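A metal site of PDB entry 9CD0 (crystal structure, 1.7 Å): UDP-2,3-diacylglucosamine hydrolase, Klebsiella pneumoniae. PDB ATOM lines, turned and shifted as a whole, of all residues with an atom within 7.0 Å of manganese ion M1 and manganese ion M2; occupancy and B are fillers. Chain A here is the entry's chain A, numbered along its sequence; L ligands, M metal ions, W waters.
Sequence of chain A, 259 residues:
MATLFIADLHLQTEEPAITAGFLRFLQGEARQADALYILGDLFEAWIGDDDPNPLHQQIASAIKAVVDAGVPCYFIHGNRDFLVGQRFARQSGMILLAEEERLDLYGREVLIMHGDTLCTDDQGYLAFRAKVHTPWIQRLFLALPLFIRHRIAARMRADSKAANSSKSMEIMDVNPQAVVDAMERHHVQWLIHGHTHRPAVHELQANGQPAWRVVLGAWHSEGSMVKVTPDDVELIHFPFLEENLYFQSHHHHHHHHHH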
ATOM      1  N   ALA A   7      26.473 -19.994  21.527  1.00  0.00           N
ATOM      2  CA  ALA A   7      25.759 -21.242  21.258  1.00  0.00           C
ATOM      3  C   ALA A   7      24.809 -21.514  22.414  1.00  0.00           C
ATOM      4  O   ALA A   7      24.902 -20.902  23.491  1.00  0.00           O
ATOM      5  CB  ALA A   7      26.729 -22.427  21.053  1.00  0.00           C
ATOM      6  N   ASP A   8      23.872 -22.465  22.202  1.00  0.00           N
ATOM      7  CA  ASP A   8      23.093 -22.961  23.292  1.00  0.00           C
ATOM      8  C   ASP A   8      22.307 -21.861  24.021  1.00  0.00           C
ATOM      9  O   ASP A   8      22.132 -21.903  25.249  1.00  0.00           O
ATOM     10  CB  ASP A   8      24.013 -23.726  24.241  1.00  0.00           C
ATOM     11  CG  ASP A   8      24.659 -24.911  23.501  1.00  0.00           C
ATOM     12  OD1 ASP A   8      23.878 -25.776  23.113  1.00  0.00           O
ATOM     13  OD2 ASP A   8      25.886 -24.925  23.263  1.00  0.00           O
ATOM     14  N   LEU A   9      21.731 -20.986  23.255  1.00  0.00           N
ATOM     15  CA  LEU A   9      20.773 -20.019  23.800  1.00  0.00           C
ATOM     16  C   LEU A   9      19.433 -20.685  24.071  1.00  0.00           C
ATOM     17  O   LEU A   9      18.767 -20.342  25.063  1.00  0.00           O
ATOM     18  CB  LEU A   9      20.570 -18.882  22.807  1.00  0.00           C
ATOM     19  CG  LEU A   9      21.775 -17.907  22.737  1.00  0.00           C
ATOM     20  CD1 LEU A   9      22.847 -18.428  21.725  1.00  0.00           C
ATOM     21  CD2 LEU A   9      21.255 -16.492  22.342  1.00  0.00           C
ATOM     22  N   HIS A  10      19.073 -21.696  23.291  1.00  0.00           N
ATOM     23  CA  HIS A  10      17.827 -22.451  23.481  1.00  0.00           C
ATOM     24  C   HIS A  10      16.634 -21.499  23.610  1.00  0.00           C
ATOM     25  O   HIS A  10      15.806 -21.612  24.529  1.00  0.00           O
ATOM     26  CB  HIS A  10      17.932 -23.402  24.711  1.00  0.00           C
ATOM     27  CG  HIS A  10      18.881 -24.560  24.520  1.00  0.00           C
ATOM     28  ND1 HIS A  10      18.463 -25.810  24.108  1.00  0.00           N
ATOM     29  CD2 HIS A  10      20.232 -24.616  24.556  1.00  0.00           C
ATOM     30  CE1 HIS A  10      19.519 -26.606  23.995  1.00  0.00           C
ATOM     31  NE2 HIS A  10      20.599 -25.908  24.271  1.00  0.00           N
ATOM     32  N   LEU A  39      26.992 -21.246  17.097  1.00  0.00           N
ATOM     33  CA  LEU A  39      27.356 -22.662  16.933  1.00  0.00           C
ATOM     34  C   LEU A  39      26.242 -23.609  17.389  1.00  0.00           C
ATOM     35  O   LEU A  39      26.510 -24.587  18.099  1.00  0.00           O
ATOM     36  CB  LEU A  39      28.656 -22.960  17.701  1.00  0.00           C
ATOM     37  CG  LEU A  39      29.832 -22.076  17.245  1.00  0.00           C
ATOM     38  CD1 LEU A  39      31.168 -22.597  17.914  1.00  0.00           C
ATOM     39  CD2 LEU A  39      30.013 -22.009  15.678  1.00  0.00           C
ATOM     40  N   GLY A  40      25.009 -23.368  16.943  1.00  0.00           N
ATOM     41  CA  GLY A  40      23.954 -24.366  17.183  1.00  0.00           C
ATOM     42  C   GLY A  40      23.136 -24.133  18.450  1.00  0.00           C
ATOM     43  O   GLY A  40      23.569 -23.506  19.402  1.00  0.00           O
ATOM     44  N   ASP A  41      21.917 -24.705  18.460  1.00  0.00           N
ATOM     45  CA  ASP A  41      20.968 -24.547  19.567  1.00  0.00           C
ATOM     46  C   ASP A  41      20.701 -23.063  19.861  1.00  0.00           C
ATOM     47  O   ASP A  41      20.612 -22.619  21.019  1.00  0.00           O
ATOM     48  CB  ASP A  41      21.417 -25.304  20.837  1.00  0.00           C
ATOM     49  CG  ASP A  41      21.411 -26.823  20.655  1.00  0.00           C
ATOM     50  OD1 ASP A  41      20.996 -27.319  19.562  1.00  0.00           O
ATOM     51  OD2 ASP A  41      21.854 -27.458  21.627  1.00  0.00           O
ATOM     52  N   GLU A  44      15.345 -23.474  21.090  1.00  0.00           N
ATOM     53  CA  GLU A  44      15.006 -24.699  21.798  1.00  0.00           C
ATOM     54  C   GLU A  44      14.380 -25.752  20.877  1.00  0.00           C
ATOM     55  O   GLU A  44      14.490 -26.958  21.142  1.00  0.00           O
ATOM     56  CB  GLU A  44      14.043 -24.359  22.947  1.00  0.00           C
ATOM     57  CG  GLU A  44      13.507 -25.629  23.703  1.00  0.00           C
ATOM     58  CD  GLU A  44      14.524 -26.441  24.459  1.00  0.00           C
ATOM     59  OE1 GLU A  44      15.692 -26.035  24.571  1.00  0.00           O
ATOM     60  OE2 GLU A  44      14.142 -27.503  24.977  1.00  0.00           O
ATOM     61  N   GLY A  78      22.495 -26.971  15.603  1.00  0.00           N
ATOM     62  CA  GLY A  78      22.565 -27.789  16.808  1.00  0.00           C
ATOM     63  C   GLY A  78      21.667 -29.023  16.695  1.00  0.00           C
ATOM     64  O   GLY A  78      21.013 -29.263  15.702  1.00  0.00           O
ATOM     65  N   ASN A  79      21.645 -29.818  17.775  1.00  0.00           N
ATOM     66  CA  ASN A  79      20.689 -30.933  17.826  1.00  0.00           C
ATOM     67  C   ASN A  79      19.247 -30.455  17.985  1.00  0.00           C
ATOM     68  O   ASN A  79      18.319 -31.208  17.649  1.00  0.00           O
ATOM     69  CB  ASN A  79      21.098 -31.882  18.953  1.00  0.00           C
ATOM     70  CG  ASN A  79      21.085 -31.219  20.315  1.00  0.00           C
ATOM     71  OD1 ASN A  79      21.905 -30.378  20.563  1.00  0.00           O
ATOM     72  ND2 ASN A  79      20.183 -31.627  21.185  1.00  0.00           N
ATOM     73  N   ARG A  80      19.040 -29.253  18.524  1.00  0.00           N
ATOM     74  CA  ARG A  80      17.669 -28.767  18.673  1.00  0.00           C
ATOM     75  C   ARG A  80      17.146 -28.182  17.353  1.00  0.00           C
ATOM     76  O   ARG A  80      15.970 -28.399  17.013  1.00  0.00           O
ATOM     77  CB  ARG A  80      17.537 -27.721  19.787  1.00  0.00           C
ATOM     78  CG  ARG A  80      18.070 -28.191  21.126  1.00  0.00           C
ATOM     79  CD  ARG A  80      17.367 -29.466  21.601  1.00  0.00           C
ATOM     80  NE  ARG A  80      15.933 -29.250  21.771  1.00  0.00           N
ATOM     81  CZ  ARG A  80      15.130 -30.048  22.474  1.00  0.00           C
ATOM     82  NH1 ARG A  80      15.548 -31.175  23.014  1.00  0.00           N
ATOM     83  NH2 ARG A  80      13.856 -29.695  22.647  1.00  0.00           N
ATOM     84  N   HIS A 114      29.020 -27.705  16.483  1.00  0.00           N
ATOM     85  CA  HIS A 114      28.124 -27.621  17.639  1.00  0.00           C
ATOM     86  C   HIS A 114      28.687 -28.430  18.814  1.00  0.00           C
ATOM     87  O   HIS A 114      28.620 -27.975  19.957  1.00  0.00           O
ATOM     88  CB  HIS A 114      26.707 -28.133  17.311  1.00  0.00           C
ATOM     89  CG  HIS A 114      25.781 -28.045  18.473  1.00  0.00           C
ATOM     90  ND1 HIS A 114      25.464 -26.854  19.100  1.00  0.00           N
ATOM     91  CD2 HIS A 114      25.116 -29.026  19.135  1.00  0.00           C
ATOM     92  CE1 HIS A 114      24.614 -27.121  20.104  1.00  0.00           C
ATOM     93  NE2 HIS A 114      24.401 -28.430  20.145  1.00  0.00           N
ATOM     94  N   GLY A 115      29.207 -29.635  18.535  1.00  0.00           N
ATOM     95  CA  GLY A 115      29.874 -30.507  19.488  1.00  0.00           C
ATOM     96  C   GLY A 115      29.118 -31.785  19.772  1.00  0.00           C
ATOM     97  O   GLY A 115      29.687 -32.704  20.392  1.00  0.00           O
ATOM     98  N   ASP A 116      27.860 -31.893  19.340  1.00  0.00           N
ATOM     99  CA  ASP A 116      27.146 -33.141  19.625  1.00  0.00           C
ATOM    100  C   ASP A 116      27.789 -34.336  18.911  1.00  0.00           C
ATOM    101  O   ASP A 116      27.704 -35.479  19.416  1.00  0.00           O
ATOM    102  CB  ASP A 116      25.663 -33.049  19.213  1.00  0.00           C
ATOM    103  CG  ASP A 116      25.483 -32.675  17.763  1.00  0.00           C
ATOM    104  OD1 ASP A 116      26.065 -31.675  17.340  1.00  0.00           O
ATOM    105  OD2 ASP A 116      24.818 -33.422  17.017  1.00  0.00           O
ATOM    106  N   TYR A 125      21.481 -40.954  21.568  1.00  0.00           N
ATOM    107  CA  TYR A 125      21.458 -39.672  20.857  1.00  0.00           C
ATOM    108  C   TYR A 125      21.931 -39.860  19.418  1.00  0.00           C
ATOM    109  O   TYR A 125      21.349 -39.308  18.495  1.00  0.00           O
ATOM    110  CB  TYR A 125      22.350 -38.613  21.565  1.00  0.00           C
ATOM    111  CG  TYR A 125      22.463 -37.435  20.644  1.00  0.00           C
ATOM    112  CD1 TYR A 125      21.333 -36.749  20.290  1.00  0.00           C
ATOM    113  CD2 TYR A 125      23.664 -37.124  19.990  1.00  0.00           C
ATOM    114  CE1 TYR A 125      21.347 -35.710  19.366  1.00  0.00           C
ATOM    115  CE2 TYR A 125      23.725 -36.079  19.067  1.00  0.00           C
ATOM    116  CZ  TYR A 125      22.544 -35.381  18.764  1.00  0.00           C
ATOM    117  OH  TYR A 125      22.524 -34.366  17.842  1.00  0.00           O
ATOM    118  N   ILE A 171      22.985 -33.811  29.525  1.00  0.00           N
ATOM    119  CA  ILE A 171      23.614 -33.970  28.215  1.00  0.00           C
ATOM    120  C   ILE A 171      24.937 -34.680  28.411  1.00  0.00           C
ATOM    121  O   ILE A 171      25.731 -34.301  29.284  1.00  0.00           O
ATOM    122  CB  ILE A 171      23.822 -32.604  27.534  1.00  0.00           C
ATOM    123  CG1 ILE A 171      22.467 -31.866  27.382  1.00  0.00           C
ATOM    124  CG2 ILE A 171      24.631 -32.719  26.264  1.00  0.00           C
ATOM    125  CD1 ILE A 171      22.607 -30.402  27.039  1.00  0.00           C
ATOM    126  N   GLY A 194      29.904 -25.997  21.377  1.00  0.00           N
ATOM    127  CA  GLY A 194      28.988 -25.897  22.491  1.00  0.00           C
ATOM    128  C   GLY A 194      28.403 -27.246  22.795  1.00  0.00           C
ATOM    129  O   GLY A 194      29.147 -28.214  23.033  1.00  0.00           O
ATOM    130  N   HIS A 195      27.051 -27.320  22.809  1.00  0.00           N
ATOM    131  CA  HIS A 195      26.298 -28.544  23.098  1.00  0.00           C
ATOM    132  C   HIS A 195      26.368 -29.103  24.519  1.00  0.00           C
ATOM    133  O   HIS A 195      25.316 -29.426  25.082  1.00  0.00           O
ATOM    134  CB  HIS A 195      26.670 -29.661  22.119  1.00  0.00           C
ATOM    135  CG  HIS A 195      25.832 -30.908  22.305  1.00  0.00           C
ATOM    136  ND1 HIS A 195      24.483 -30.922  22.039  1.00  0.00           N
ATOM    137  CD2 HIS A 195      26.122 -32.139  22.797  1.00  0.00           C
ATOM    138  CE1 HIS A 195      23.983 -32.116  22.319  1.00  0.00           C
ATOM    139  NE2 HIS A 195      24.959 -32.880  22.761  1.00  0.00           N
ATOM    140  N   THR A 196      27.575 -29.270  25.118  1.00  0.00           N
ATOM    141  CA  THR A 196      27.640 -29.948  26.411  1.00  0.00           C
ATOM    142  C   THR A 196      27.310 -29.060  27.594  1.00  0.00           C
ATOM    143  O   THR A 196      27.135 -29.598  28.702  1.00  0.00           O
ATOM    144  CB  THR A 196      29.038 -30.532  26.626  1.00  0.00           C
ATOM    145  OG1 THR A 196      29.982 -29.450  26.666  1.00  0.00           O
ATOM    146  CG2 THR A 196      29.397 -31.425  25.438  1.00  0.00           C
ATOM    147  N   HIS A 197      27.218 -27.714  27.382  1.00  0.00           N
ATOM    148  CA  HIS A 197      26.766 -26.785  28.427  1.00  0.00           C
ATOM    149  C   HIS A 197      27.747 -26.773  29.606  1.00  0.00           C
ATOM    150  O   HIS A 197      27.357 -26.586  30.776  1.00  0.00           O
ATOM    151  CB  HIS A 197      25.341 -27.122  28.897  1.00  0.00           C
ATOM    152  CG  HIS A 197      24.280 -26.978  27.816  1.00  0.00           C
ATOM    153  ND1 HIS A 197      22.922 -27.107  28.083  1.00  0.00           N
ATOM    154  CD2 HIS A 197      24.380 -26.699  26.498  1.00  0.00           C
ATOM    155  CE1 HIS A 197      22.246 -26.945  26.953  1.00  0.00           C
ATOM    156  NE2 HIS A 197      23.107 -26.699  25.989  1.00  0.00           N
ATOM    157  N   ALA A 218      25.683 -22.599  27.966  1.00  0.00           N
ATOM    158  CA  ALA A 218      24.274 -22.340  27.715  1.00  0.00           C
ATOM    159  C   ALA A 218      23.834 -21.037  28.359  1.00  0.00           C
ATOM    160  O   ALA A 218      24.359 -20.588  29.388  1.00  0.00           O
ATOM    161  CB  ALA A 218      23.375 -23.483  28.242  1.00  0.00           C
HETATM  162  C1  LIG L   1      10.360 -32.991  15.905  1.00  0.00           C
HETATM  163  C2  LIG L   1      12.988 -32.358  19.940  1.00  0.00           C
HETATM  164  C3  LIG L   1      15.237 -33.163  20.231  1.00  0.00           C
HETATM  165  C4  LIG L   1      17.353 -34.291  21.040  1.00  0.00           C
HETATM  166  C5  LIG L   1      17.450 -36.753  21.210  1.00  0.00           C
HETATM  167  C6  LIG L   1      18.766 -37.872  22.856  1.00  0.00           C
HETATM  168  C7  LIG L   1      18.772 -35.468  22.807  1.00  0.00           C
HETATM  169  C8  LIG L   1      12.352 -34.884  11.930  1.00  0.00           C
HETATM  170  C9  LIG L   1      11.382 -34.129  13.843  1.00  0.00           C
HETATM  171  C10 LIG L   1      12.119 -31.861  14.516  1.00  0.00           C
HETATM  172  C11 LIG L   1      12.794 -31.433  15.815  1.00  0.00           C
HETATM  173  C12 LIG L   1      11.098 -32.547  17.173  1.00  0.00           C
HETATM  174  C13 LIG L   1      13.512 -31.458  19.018  1.00  0.00           C
HETATM  175  C14 LIG L   1      13.882 -33.240  20.540  1.00  0.00           C
HETATM  176  C15 LIG L   1      15.786 -32.295  19.263  1.00  0.00           C
HETATM  177  C16 LIG L   1      14.875 -31.423  18.656  1.00  0.00           C
HETATM  178  C17 LIG L   1      17.874 -35.507  21.750  1.00  0.00           C
HETATM  179  C18 LIG L   1      17.897 -37.948  21.781  1.00  0.00           C
HETATM  180  C19 LIG L   1      19.188 -36.646  23.366  1.00  0.00           C
HETATM  181  C20 LIG L   1      18.329 -34.205  26.060  1.00  0.00           C
HETATM  182  C21 LIG L   1      20.722 -34.075  23.542  1.00  0.00           C
HETATM  183  C22 LIG L   1      14.935 -35.114  21.559  1.00  0.00           C
HETATM  184  C23 LIG L   1      13.682 -34.298  21.607  1.00  0.00           C
HETATM  185  C24 LIG L   1      10.557 -35.279  13.999  1.00  0.00           C
HETATM  186  C25 LIG L   1      10.698 -36.197  13.023  1.00  0.00           C
HETATM  187  C26 LIG L   1      11.600 -36.066  11.969  1.00  0.00           C
HETATM  188  C27 LIG L   1       9.843 -37.483  13.117  1.00  0.00           C
HETATM  189  F1  LIG L   1       8.658 -37.209  13.485  1.00  0.00           F
HETATM  190  F2  LIG L   1       9.881 -38.107  12.000  1.00  0.00           F
HETATM  191  F3  LIG L   1      10.295 -38.220  14.000  1.00  0.00           F
HETATM  192  N1  LIG L   1      12.198 -33.965  12.836  1.00  0.00           N
HETATM  193  N2  LIG L   1      11.310 -33.083  14.784  1.00  0.00           N
HETATM  194  N3  LIG L   1      11.825 -31.279  16.851  1.00  0.00           N
HETATM  195  N4  LIG L   1      15.920 -34.206  20.980  1.00  0.00           N
HETATM  196  N5  LIG L   1      19.265 -34.270  23.407  1.00  0.00           N
HETATM  197  O1  LIG L   1      11.265 -30.266  19.064  1.00  0.00           O
HETATM  198  O2  LIG L   1      12.917 -29.249  17.719  1.00  0.00           O
HETATM  199  O3  LIG L   1      18.096 -33.496  20.548  1.00  0.00           O
HETATM  200  O4  LIG L   1      18.618 -32.043  24.444  1.00  0.00           O
HETATM  201  O5  LIG L   1      16.861 -33.567  23.938  1.00  0.00           O
HETATM  202  S1  LIG L   1      12.300 -30.416  18.214  1.00  0.00           S
HETATM  203  S2  LIG L   1      18.235 -33.451  24.412  1.00  0.00           S
HETATM  204 CL1  LIG L   1      13.489 -34.606  10.611  1.00  0.00          CL
HETATM  205 MN    MN M   1      22.428 -26.893  23.918  1.00  0.00          MN
HETATM  206 MN    MN M   2      23.084 -29.202  21.677  1.00  0.00          MN
HETATM  207  O   HOH W   1      22.798 -28.838  23.600  1.00  0.00           O
HETATM  208  O   HOH W   2      20.461 -30.028  23.722  1.00  0.00           O
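ND2 of Asn 79 sits at hydrogen-bond distance from O3 of the ligand (2.9 Å). NH1 of Arg 80 lies within hydrogen-bond range of O5 of the ligand (2.9 Å).
A ring nitrogen (ND1) of His 10 sits at hydrogen-bond distance from the side-chain carboxylate (OE1) of Glu 44, at 2.8 Å. A ring nitrogen (ND1) of His 114 lies within hydrogen-bond range of the backbone carbonyl oxygen (O) of Leu 39, 2.7 Å away. The backbone carbonyl oxygen (O) of Gly 40 is in hydrogen-bond range of the backbone NH (N) of Asp 8 (3.0 Å). The backbone carbonyl oxygen (O) of His 114 sits at hydrogen-bond distance from the backbone NH (N) of Gly 194 (2.8 Å). O of Asp 41 is in hydrogen-bond range of N of Leu 9, 3.0 Å away. The backbone NH (N) of Arg 80 lies within hydrogen-bond range of the side-chain carboxylate (OD1) of Asp 41, 2.9 Å away. OD2 of Asp 8 lies within hydrogen-bond range of N of His 195 (2.7 Å).
Of the 21 residues printed, 4 come within 4 Å of manganese ion M1. The nearest printed residue that does not touch manganese ion M1 is His 195 (4.01 Å).
Of the 21 residues printed, 5 come within 4 Å of manganese ion M2. The nearest printed residue that does not touch manganese ion M2 is His 10 (4.9 Å).
Manganese ion M1 is bound by OD1 of Asp 8 (2.0 Å), water W1 (2.0 Å), NE2 of His 10 (2.1 Å), NE2 of His 197 (2.2 Å) and OD2 of Asp 41 (2.4 Å). Manganese ion M1 has five donor atoms within binding distance.
Manganese ion M2 is bound by water W1 (2.0 Å), the side-chain amide oxygen of Asn 79 (2.0 Å), the side-chain carboxylate of Asp 41 (2.1 Å), a ring nitrogen (NE2) of His 114 (2.2 Å) and a ring nitrogen (ND1) of His 195 (2.2 Å).
Water W2 bridges an oxygen (O4) of the ligand and the side-chain amide nitrogen of Asn 79.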
